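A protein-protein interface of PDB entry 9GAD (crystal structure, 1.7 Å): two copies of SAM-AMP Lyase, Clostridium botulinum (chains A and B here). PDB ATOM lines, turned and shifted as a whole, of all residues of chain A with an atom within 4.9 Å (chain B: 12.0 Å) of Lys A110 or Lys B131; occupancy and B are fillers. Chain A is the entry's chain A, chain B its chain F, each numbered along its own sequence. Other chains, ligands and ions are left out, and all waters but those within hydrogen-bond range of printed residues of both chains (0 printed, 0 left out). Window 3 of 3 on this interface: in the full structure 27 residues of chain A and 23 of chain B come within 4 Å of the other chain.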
ATOM      1  N   ALA A 106      -4.708  19.650  11.707  1.00  0.00           N
ATOM      2  CA  ALA A 106      -4.196  20.999  11.792  1.00  0.00           C
ATOM      3  C   ALA A 106      -5.125  21.894  12.609  1.00  0.00           C
ATOM      4  O   ALA A 106      -4.660  22.682  13.444  1.00  0.00           O
ATOM      5  CB  ALA A 106      -4.006  21.544  10.385  1.00  0.00           C
ATOM      6  N   LYS A 107      -6.431  21.794  12.343  1.00  0.00           N
ATOM      7  CA  LYS A 107      -7.420  22.551  13.093  1.00  0.00           C
ATOM      8  C   LYS A 107      -7.429  22.161  14.574  1.00  0.00           C
ATOM      9  O   LYS A 107      -7.564  23.021  15.459  1.00  0.00           O
ATOM     10  CB  LYS A 107      -8.814  22.404  12.472  1.00  0.00           C
ATOM     11  CG  LYS A 107      -8.948  23.130  11.139  1.00  0.00           C
ATOM     12  CD  LYS A 107     -10.272  22.835  10.452  1.00  0.00           C
ATOM     13  CE  LYS A 107     -10.396  23.472   9.137  1.00  0.00           C
ATOM     14  NZ  LYS A 107     -11.618  22.987   8.464  1.00  0.00           N
ATOM     15  N   GLU A 108      -7.343  20.854  14.846  1.00  0.00           N
ATOM     16  CA  GLU A 108      -7.311  20.370  16.227  1.00  0.00           C
ATOM     17  C   GLU A 108      -6.070  20.884  16.954  1.00  0.00           C
ATOM     18  O   GLU A 108      -6.141  21.243  18.132  1.00  0.00           O
ATOM     19  CB  GLU A 108      -7.422  18.848  16.220  1.00  0.00           C
ATOM     20  CG  GLU A 108      -7.474  18.192  17.600  1.00  0.00           C
ATOM     21  CD  GLU A 108      -8.604  18.631  18.521  1.00  0.00           C
ATOM     22  OE1 GLU A 108      -8.489  18.425  19.740  1.00  0.00           O
ATOM     23  OE2 GLU A 108      -9.617  19.121  18.023  1.00  0.00           O
ATOM     24  N   LEU A 109      -4.909  20.920  16.269  1.00  0.00           N
ATOM     25  CA  LEU A 109      -3.697  21.406  16.905  1.00  0.00           C
ATOM     26  C   LEU A 109      -3.835  22.892  17.214  1.00  0.00           C
ATOM     27  O   LEU A 109      -3.362  23.372  18.260  1.00  0.00           O
ATOM     28  CB  LEU A 109      -2.480  21.159  16.003  1.00  0.00           C
ATOM     29  CG  LEU A 109      -1.123  21.524  16.623  1.00  0.00           C
ATOM     30  CD1 LEU A 109      -0.779  20.650  17.796  1.00  0.00           C
ATOM     31  CD2 LEU A 109      -0.014  21.364  15.554  1.00  0.00           C
ATOM     32  N   LYS A 110      -4.454  23.639  16.292  1.00  0.00           N
ATOM     33  CA  LYS A 110      -4.666  25.067  16.476  1.00  0.00           C
ATOM     34  C   LYS A 110      -5.455  25.315  17.781  1.00  0.00           C
ATOM     35  O   LYS A 110      -5.112  26.221  18.548  1.00  0.00           O
ATOM     36  CB  LYS A 110      -5.420  25.651  15.276  1.00  0.00           C
ATOM     37  CG  LYS A 110      -5.691  27.150  15.367  1.00  0.00           C
ATOM     38  CD  LYS A 110      -6.615  27.622  14.227  1.00  0.00           C
ATOM     39  CE  LYS A 110      -6.981  29.055  14.256  1.00  0.00           C
ATOM     40  NZ  LYS A 110      -7.662  29.510  15.477  1.00  0.00           N
ATOM     41  N   ASN A 111      -6.482  24.490  17.988  1.00  0.00           N
ATOM     42  CA  ASN A 111      -7.330  24.534  19.181  1.00  0.00           C
ATOM     43  C   ASN A 111      -6.541  24.167  20.449  1.00  0.00           C
ATOM     44  O   ASN A 111      -6.537  24.923  21.416  1.00  0.00           O
ATOM     45  CB  ASN A 111      -8.522  23.608  19.008  1.00  0.00           C
ATOM     46  CG  ASN A 111      -9.680  24.247  18.279  1.00  0.00           C
ATOM     47  OD1 ASN A 111      -9.667  25.453  17.988  1.00  0.00           O
ATOM     48  ND2 ASN A 111     -10.693  23.444  17.984  1.00  0.00           N
ATOM     49  N   GLN A 112      -5.866  23.018  20.440  1.00  0.00           N
ATOM     50  CA  GLN A 112      -5.118  22.537  21.601  1.00  0.00           C
ATOM     51  C   GLN A 112      -4.022  23.497  22.045  1.00  0.00           C
ATOM     52  O   GLN A 112      -3.745  23.606  23.252  1.00  0.00           O
ATOM     53  CB  GLN A 112      -4.379  21.218  21.332  1.00  0.00           C
ATOM     54  CG  GLN A 112      -5.281  20.013  21.102  1.00  0.00           C
ATOM     55  CD  GLN A 112      -5.923  19.504  22.395  1.00  0.00           C
ATOM     56  OE1 GLN A 112      -5.371  19.640  23.497  1.00  0.00           O
ATOM     57  NE2 GLN A 112      -7.160  19.063  22.287  1.00  0.00           N
ATOM     58  N   MET A 113      -3.359  24.164  21.071  1.00  0.00           N
ATOM     59  CA  MET A 113      -2.270  25.073  21.390  1.00  0.00           C
ATOM     60  C   MET A 113      -2.783  26.484  21.622  1.00  0.00           C
ATOM     61  O   MET A 113      -1.993  27.408  21.847  1.00  0.00           O
ATOM     62  CB  MET A 113      -1.207  25.064  20.276  1.00  0.00           C
ATOM     63  CG  MET A 113      -0.584  23.699  19.998  1.00  0.00           C
ATOM     64  SD  MET A 113       0.157  22.917  21.440  1.00  0.00           S
ATOM     65  CE  MET A 113       1.375  24.174  21.835  1.00  0.00           C
ATOM     66  N   LYS A 114      -4.099  26.678  21.502  1.00  0.00           N
ATOM     67  CA  LYS A 114      -4.747  27.977  21.668  1.00  0.00           C
ATOM     68  C   LYS A 114      -4.084  29.038  20.806  1.00  0.00           C
ATOM     69  O   LYS A 114      -3.760  30.126  21.257  1.00  0.00           O
ATOM     70  CB  LYS A 114      -4.890  28.270  23.173  1.00  0.00           C
ATOM     71  CG  LYS A 114      -6.107  27.567  23.757  1.00  0.00           C
ATOM     72  CD  LYS A 114      -5.986  26.792  25.064  1.00  0.00           C
ATOM     73  CE  LYS A 114      -7.091  25.775  25.138  1.00  0.00           C
ATOM     74  NZ  LYS A 114      -7.272  25.312  26.514  1.00  0.00           N
ATOM     75  N   GLN A 115      -3.973  28.734  19.502  1.00  0.00           N
ATOM     76  CA  GLN A 115      -3.347  29.639  18.558  1.00  0.00           C
ATOM     77  C   GLN A 115      -4.418  30.429  17.800  1.00  0.00           C
ATOM     78  O   GLN A 115      -5.447  29.839  17.451  1.00  0.00           O
ATOM     79  CB  GLN A 115      -2.548  28.807  17.544  1.00  0.00           C
ATOM     80  CG  GLN A 115      -1.379  28.053  18.173  1.00  0.00           C
ATOM     81  CD  GLN A 115      -0.339  28.982  18.767  1.00  0.00           C
ATOM     82  OE1 GLN A 115       0.270  29.777  18.049  1.00  0.00           O
ATOM     83  NE2 GLN A 115      -0.140  28.945  20.084  1.00  0.00           N
ATOM     84  N   SER A 116      -4.146  31.718  17.547  1.00  0.00           N
ATOM     85  CA  SER A 116      -5.083  32.583  16.839  1.00  0.00           C
ATOM     86  C   SER A 116      -5.120  32.251  15.350  1.00  0.00           C
ATOM     87  O   SER A 116      -6.176  32.338  14.725  1.00  0.00           O
ATOM     88  CB  SER A 116      -4.767  34.045  17.048  1.00  0.00           C
ATOM     89  OG  SER A 116      -4.875  34.371  18.428  1.00  0.00           O
ATOM     90  N   THR A 117      -3.951  31.896  14.797  1.00  0.00           N
ATOM     91  CA  THR A 117      -3.805  31.540  13.387  1.00  0.00           C
ATOM     92  C   THR A 117      -2.887  30.322  13.264  1.00  0.00           C
ATOM     93  O   THR A 117      -2.068  30.062  14.172  1.00  0.00           O
ATOM     94  CB  THR A 117      -3.261  32.712  12.564  1.00  0.00           C
ATOM     95  OG1 THR A 117      -1.877  32.864  12.903  1.00  0.00           O
ATOM     96  CG2 THR A 117      -3.994  34.022  12.793  1.00  0.00           C
ATOM     97  N   LEU A 118      -3.009  29.586  12.147  1.00  0.00           N
ATOM     98  CA  LEU A 118      -2.143  28.425  11.900  1.00  0.00           C
ATOM     99  C   LEU A 118      -2.046  28.186  10.392  1.00  0.00           C
ATOM    100  O   LEU A 118      -3.023  28.372   9.680  1.00  0.00           O
ATOM    101  CB  LEU A 118      -2.655  27.187  12.648  1.00  0.00           C
ATOM    102  CG  LEU A 118      -1.807  25.909  12.515  1.00  0.00           C
ATOM    103  CD1 LEU A 118      -1.679  25.141  13.830  1.00  0.00           C
ATOM    104  CD2 LEU A 118      -2.405  24.974  11.468  1.00  0.00           C
ATOM    105  N   ALA B   2     -16.731  27.946  18.277  1.00  0.00           N
ATOM    106  CA  ALA B   2     -16.297  29.309  17.889  1.00  0.00           C
ATOM    107  C   ALA B   2     -16.341  29.432  16.363  1.00  0.00           C
ATOM    108  O   ALA B   2     -16.181  28.445  15.649  1.00  0.00           O
ATOM    109  CB  ALA B   2     -14.906  29.599  18.445  1.00  0.00           C
ATOM    110  N   ASN B   3     -16.543  30.660  15.879  1.00  0.00           N
ATOM    111  CA  ASN B   3     -16.447  30.990  14.462  1.00  0.00           C
ATOM    112  C   ASN B   3     -15.032  30.707  13.940  1.00  0.00           C
ATOM    113  O   ASN B   3     -14.074  30.634  14.715  1.00  0.00           O
ATOM    114  CB  ASN B   3     -16.811  32.448  14.239  1.00  0.00           C
ATOM    115  CG  ASN B   3     -18.216  32.797  14.712  1.00  0.00           C
ATOM    116  OD1 ASN B   3     -18.947  31.969  15.280  1.00  0.00           O
ATOM    117  ND2 ASN B   3     -18.625  34.025  14.458  1.00  0.00           N
ATOM    118  N   ALA B   4     -14.907  30.540  12.620  1.00  0.00           N
ATOM    119  CA  ALA B   4     -13.665  30.076  11.998  1.00  0.00           C
ATOM    120  C   ALA B   4     -13.639  30.445  10.514  1.00  0.00           C
ATOM    121  O   ALA B   4     -14.668  30.567   9.843  1.00  0.00           O
ATOM    122  CB  ALA B   4     -13.515  28.579  12.194  1.00  0.00           C
ATOM    123  N   MET B   5     -12.436  30.636   9.985  1.00  0.00           N
ATOM    124  CA  MET B   5     -12.295  30.886   8.566  1.00  0.00           C
ATOM    125  C   MET B   5     -11.089  30.110   8.065  1.00  0.00           C
ATOM    126  O   MET B   5     -10.124  29.897   8.815  1.00  0.00           O
ATOM    127  CB  MET B   5     -12.272  32.385   8.243  1.00  0.00           C
ATOM    128  CG  MET B   5     -11.100  33.154   8.700  1.00  0.00           C
ATOM    129  SD  MET B   5     -11.503  34.886   8.393  1.00  0.00           S
ATOM    130  CE  MET B   5     -12.390  35.274   9.913  1.00  0.00           C
ATOM    131  N   ALA B   6     -11.213  29.613   6.827  1.00  0.00           N
ATOM    132  CA  ALA B   6     -10.096  28.941   6.167  1.00  0.00           C
ATOM    133  C   ALA B   6      -9.959  29.429   4.719  1.00  0.00           C
ATOM    134  O   ALA B   6     -10.952  29.647   4.033  1.00  0.00           O
ATOM    135  CB  ALA B   6     -10.267  27.447   6.269  1.00  0.00           C
ATOM    136  N   HIS B   7      -8.724  29.740   4.306  1.00  0.00           N
ATOM    137  CA  HIS B   7      -8.395  30.116   2.937  1.00  0.00           C
ATOM    138  C   HIS B   7      -7.387  29.122   2.371  1.00  0.00           C
ATOM    139  O   HIS B   7      -6.445  28.759   3.081  1.00  0.00           O
ATOM    140  CB  HIS B   7      -7.901  31.567   2.832  1.00  0.00           C
ATOM    141  CG  HIS B   7      -7.511  31.936   1.434  1.00  0.00           C
ATOM    142  ND1 HIS B   7      -6.264  31.694   0.890  1.00  0.00           N
ATOM    143  CD2 HIS B   7      -8.234  32.522   0.435  1.00  0.00           C
ATOM    144  CE1 HIS B   7      -6.249  32.101  -0.384  1.00  0.00           C
ATOM    145  NE2 HIS B   7      -7.450  32.580  -0.689  1.00  0.00           N
ATOM    146  N   MET B   8      -7.582  28.682   1.113  1.00  0.00           N
ATOM    147  CA  MET B   8      -6.655  27.811   0.410  1.00  0.00           C
ATOM    148  C   MET B   8      -6.249  28.457  -0.918  1.00  0.00           C
ATOM    149  O   MET B   8      -7.107  28.909  -1.671  1.00  0.00           O
ATOM    150  CB  MET B   8      -7.256  26.422   0.141  1.00  0.00           C
ATOM    151  CG  MET B   8      -6.462  25.541  -0.843  1.00  0.00           C
ATOM    152  SD  MET B   8      -7.283  23.999  -1.323  1.00  0.00           S
ATOM    153  CE  MET B   8      -8.626  24.602  -2.361  1.00  0.00           C
ATOM    154  N   ASN B  88       1.536  34.688   1.473  1.00  0.00           N
ATOM    155  CA  ASN B  88       0.157  34.479   1.933  1.00  0.00           C
ATOM    156  C   ASN B  88      -0.727  35.502   1.237  1.00  0.00           C
ATOM    157  O   ASN B  88      -0.508  36.700   1.376  1.00  0.00           O
ATOM    158  CB  ASN B  88       0.116  34.563   3.451  1.00  0.00           C
ATOM    159  CG  ASN B  88      -1.216  34.225   4.083  1.00  0.00           C
ATOM    160  OD1 ASN B  88      -2.279  34.420   3.487  1.00  0.00           O
ATOM    161  ND2 ASN B  88      -1.169  33.799   5.341  1.00  0.00           N
ATOM    162  N   GLU B  89      -1.709  35.012   0.467  1.00  0.00           N
ATOM    163  CA  GLU B  89      -2.552  35.864  -0.364  1.00  0.00           C
ATOM    164  C   GLU B  89      -3.313  36.894   0.474  1.00  0.00           C
ATOM    165  O   GLU B  89      -3.781  37.892  -0.061  1.00  0.00           O
ATOM    166  CB  GLU B  89      -3.479  34.981  -1.198  1.00  0.00           C
ATOM    167  CG  GLU B  89      -4.324  35.767  -2.197  1.00  0.00           C
ATOM    168  CD  GLU B  89      -4.842  34.958  -3.378  1.00  0.00           C
ATOM    169  OE1 GLU B  89      -5.361  33.839  -3.156  1.00  0.00           O
ATOM    170  OE2 GLU B  89      -4.736  35.458  -4.527  1.00  0.00           O
ATOM    171  N   GLU B  90      -3.432  36.690   1.788  1.00  0.00           N
ATOM    172  CA  GLU B  90      -4.113  37.661   2.628  1.00  0.00           C
ATOM    173  C   GLU B  90      -3.293  38.945   2.784  1.00  0.00           C
ATOM    174  O   GLU B  90      -3.860  40.004   3.037  1.00  0.00           O
ATOM    175  CB  GLU B  90      -4.455  37.122   4.009  1.00  0.00           C
ATOM    176  CG  GLU B  90      -5.238  38.155   4.814  1.00  0.00           C
ATOM    177  CD  GLU B  90      -5.948  37.600   6.017  1.00  0.00           C
ATOM    178  OE1 GLU B  90      -6.515  36.529   5.828  1.00  0.00           O
ATOM    179  OE2 GLU B  90      -5.982  38.230   7.104  1.00  0.00           O
ATOM    180  N   PHE B  91      -1.962  38.839   2.659  1.00  0.00           N
ATOM    181  CA  PHE B  91      -1.051  39.957   2.873  1.00  0.00           C
ATOM    182  C   PHE B  91      -0.321  40.346   1.580  1.00  0.00           C
ATOM    183  O   PHE B  91       0.238  41.436   1.512  1.00  0.00           O
ATOM    184  CB  PHE B  91      -0.045  39.588   3.971  1.00  0.00           C
ATOM    185  CG  PHE B  91      -0.672  39.024   5.241  1.00  0.00           C
ATOM    186  CD1 PHE B  91      -1.728  39.685   5.865  1.00  0.00           C
ATOM    187  CD2 PHE B  91      -0.236  37.811   5.786  1.00  0.00           C
ATOM    188  CE1 PHE B  91      -2.305  39.164   7.016  1.00  0.00           C
ATOM    189  CE2 PHE B  91      -0.830  37.288   6.919  1.00  0.00           C
ATOM    190  CZ  PHE B  91      -1.863  37.961   7.533  1.00  0.00           C
ATOM    191  N   VAL B  92      -0.327  39.481   0.553  1.00  0.00           N
ATOM    192  CA  VAL B  92       0.458  39.680  -0.660  1.00  0.00           C
ATOM    193  C   VAL B  92      -0.458  39.783  -1.877  1.00  0.00           C
ATOM    194  O   VAL B  92      -1.218  38.853  -2.134  1.00  0.00           O
ATOM    195  CB  VAL B  92       1.463  38.523  -0.850  1.00  0.00           C
ATOM    196  CG1 VAL B  92       2.231  38.615  -2.158  1.00  0.00           C
ATOM    197  CG2 VAL B  92       2.427  38.419   0.325  1.00  0.00           C
ATOM    198  N   LEU B 127      -1.138  26.583   0.243  1.00  0.00           N
ATOM    199  CA  LEU B 127      -1.208  27.154   1.568  1.00  0.00           C
ATOM    200  C   LEU B 127      -2.661  27.157   2.037  1.00  0.00           C
ATOM    201  O   LEU B 127      -3.533  27.792   1.414  1.00  0.00           O
ATOM    202  CB  LEU B 127      -0.654  28.575   1.609  1.00  0.00           C
ATOM    203  CG  LEU B 127      -0.805  29.314   2.937  1.00  0.00           C
ATOM    204  CD1 LEU B 127       0.012  28.588   4.025  1.00  0.00           C
ATOM    205  CD2 LEU B 127      -0.408  30.814   2.764  1.00  0.00           C
ATOM    206  N   HIS B 128      -2.898  26.494   3.188  1.00  0.00           N
ATOM    207  CA  HIS B 128      -4.161  26.637   3.914  1.00  0.00           C
ATOM    208  C   HIS B 128      -3.923  27.468   5.174  1.00  0.00           C
ATOM    209  O   HIS B 128      -3.013  27.174   5.970  1.00  0.00           O
ATOM    210  CB  HIS B 128      -4.664  25.241   4.292  1.00  0.00           C
ATOM    211  CG  HIS B 128      -4.957  24.381   3.135  1.00  0.00           C
ATOM    212  ND1 HIS B 128      -6.237  23.936   2.852  1.00  0.00           N
ATOM    213  CD2 HIS B 128      -4.180  23.853   2.193  1.00  0.00           C
ATOM    214  CE1 HIS B 128      -6.179  23.115   1.802  1.00  0.00           C
ATOM    215  NE2 HIS B 128      -4.921  23.050   1.379  1.00  0.00           N
ATOM    216  N   TYR B 129      -4.673  28.554   5.315  1.00  0.00           N
ATOM    217  CA  TYR B 129      -4.524  29.522   6.393  1.00  0.00           C
ATOM    218  C   TYR B 129      -5.791  29.517   7.244  1.00  0.00           C
ATOM    219  O   TYR B 129      -6.880  29.776   6.726  1.00  0.00           O
ATOM    220  CB  TYR B 129      -4.230  30.909   5.817  1.00  0.00           C
ATOM    221  CG  TYR B 129      -3.843  31.979   6.800  1.00  0.00           C
ATOM    222  CD1 TYR B 129      -2.920  31.742   7.822  1.00  0.00           C
ATOM    223  CD2 TYR B 129      -4.411  33.244   6.736  1.00  0.00           C
ATOM    224  CE1 TYR B 129      -2.557  32.741   8.722  1.00  0.00           C
ATOM    225  CE2 TYR B 129      -4.063  34.240   7.644  1.00  0.00           C
ATOM    226  CZ  TYR B 129      -3.138  33.987   8.636  1.00  0.00           C
ATOM    227  OH  TYR B 129      -2.756  34.992   9.480  1.00  0.00           O
ATOM    228  N   PHE B 130      -5.660  29.177   8.527  1.00  0.00           N
ATOM    229  CA  PHE B 130      -6.808  28.996   9.409  1.00  0.00           C
ATOM    230  C   PHE B 130      -6.816  30.141  10.427  1.00  0.00           C
ATOM    231  O   PHE B 130      -5.779  30.422  11.035  1.00  0.00           O
ATOM    232  CB  PHE B 130      -6.751  27.661  10.162  1.00  0.00           C
ATOM    233  CG  PHE B 130      -6.694  26.462   9.231  1.00  0.00           C
ATOM    234  CD1 PHE B 130      -7.800  26.140   8.463  1.00  0.00           C
ATOM    235  CD2 PHE B 130      -5.547  25.695   9.102  1.00  0.00           C
ATOM    236  CE1 PHE B 130      -7.770  25.052   7.593  1.00  0.00           C
ATOM    237  CE2 PHE B 130      -5.519  24.619   8.228  1.00  0.00           C
ATOM    238  CZ  PHE B 130      -6.626  24.322   7.448  1.00  0.00           C
ATOM    239  N   LYS B 131      -7.997  30.751  10.639  1.00  0.00           N
ATOM    240  CA  LYS B 131      -8.173  31.700  11.728  1.00  0.00           C
ATOM    241  C   LYS B 131      -9.470  31.438  12.530  1.00  0.00           C
ATOM    242  O   LYS B 131     -10.387  30.756  12.019  1.00  0.00           O
ATOM    243  CB  LYS B 131      -8.243  33.146  11.256  1.00  0.00           C
ATOM    244  CG  LYS B 131      -7.275  33.676  10.256  1.00  0.00           C
ATOM    245  CD  LYS B 131      -8.122  34.624   9.407  1.00  0.00           C
ATOM    246  CE  LYS B 131      -7.445  35.726   8.698  1.00  0.00           C
ATOM    247  NZ  LYS B 131      -8.438  36.380   7.836  1.00  0.00           N
ATOM    248  OXT LYS B 131      -9.501  31.895  13.687  1.00  0.00           O
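Printed residues of chain B that touch a printed residue of chain A: His B128, Tyr B129, Phe B130 and Lys B131.
Of the 13 printed residues of chain A, 5 touch a printed residue of chain B.
Printed residues of chain A that touch a printed residue of chain B: Lys A107, Lys A110, Ser A116, Thr A117 and Leu A118.
Along chain A the printed residues that touch a printed residue of chain B span positions 107 to 118.
Among the printed residues, 9 pairs touch across the chains.
Among the printed residues, no Asp or Glu carboxylate lies within 4 Å of a Lys or Arg side-chain nitrogen of the other chain.
Lys A110 touches just these residues of chain B: Phe B130 (3.7 Å) and Lys B131 (3.5 Å).
Of the printed residues of chain A, Lys B131 touches Lys A110 and Ser A116.
Asn A111 touches none of the printed residues of chain B.
No residue of chain B comes within 4 Å of Met A113.
No residue of chain B comes within 4 Å of Gln A115.
Printed residues of chain B within 4 Å of Thr A117: Tyr B129 and Phe B130.
Printed residues of chain B within 4 Å of Lys A107: Phe B130 (3.4 Å).
Of the printed residues of chain A, Phe B130 touches Lys A107, Lys A110, Thr A117 and Leu A118.
Of the printed residues of chain A, Tyr B129 touches Thr A117 and Leu A118.
Val B92 touches none of the printed residues of chain A.
Gln A112 touches none of the printed residues of chain B.
O of Lys A110 lies within hydrogen-bond range of N of Gln A115.
The side-chain amino group of Lys A110 is in hydrogen-bond range of the backbone carbonyl oxygen of Ser A116 (3.3 Å).
The chain-end carboxylate (O) of Lys B131 lies within hydrogen-bond range of the backbone NH (N) of Met B5 (2.9 Å).
The backbone carbonyl oxygen of His B7 lies within hydrogen-bond range of the backbone NH of Tyr B129, at 2.9 Å.
The side-chain sulfur (SD) of Met B8 lies close to a ring nitrogen (NE2) of His B128.
The side-chain carboxylate of Glu B90 is in salt-bridge range of the side-chain amino group of Lys B131, at 2.8 Å.
No position is printed for both chains.
Among the printed residues, merely in contact across the chains: Lys A107 with Phe B130 (3.4 Å), Lys A110 with Phe B130 (3.7 Å), Ser A116 with Lys B131 (3.5 Å), Thr A117 with Tyr B129 (3.7 Å), Thr A117 with Phe B130 (3.3 Å), Leu A118 with His B128 (3.9 Å) and Leu A118 with Tyr B129 (3.8 Å).
NZ of Lys A110 is in salt-bridge range of OXT of Lys B131 (3.5 Å).
N of Phe B130 lies within hydrogen-bond range of O of Leu A118, 3.0 Å away.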
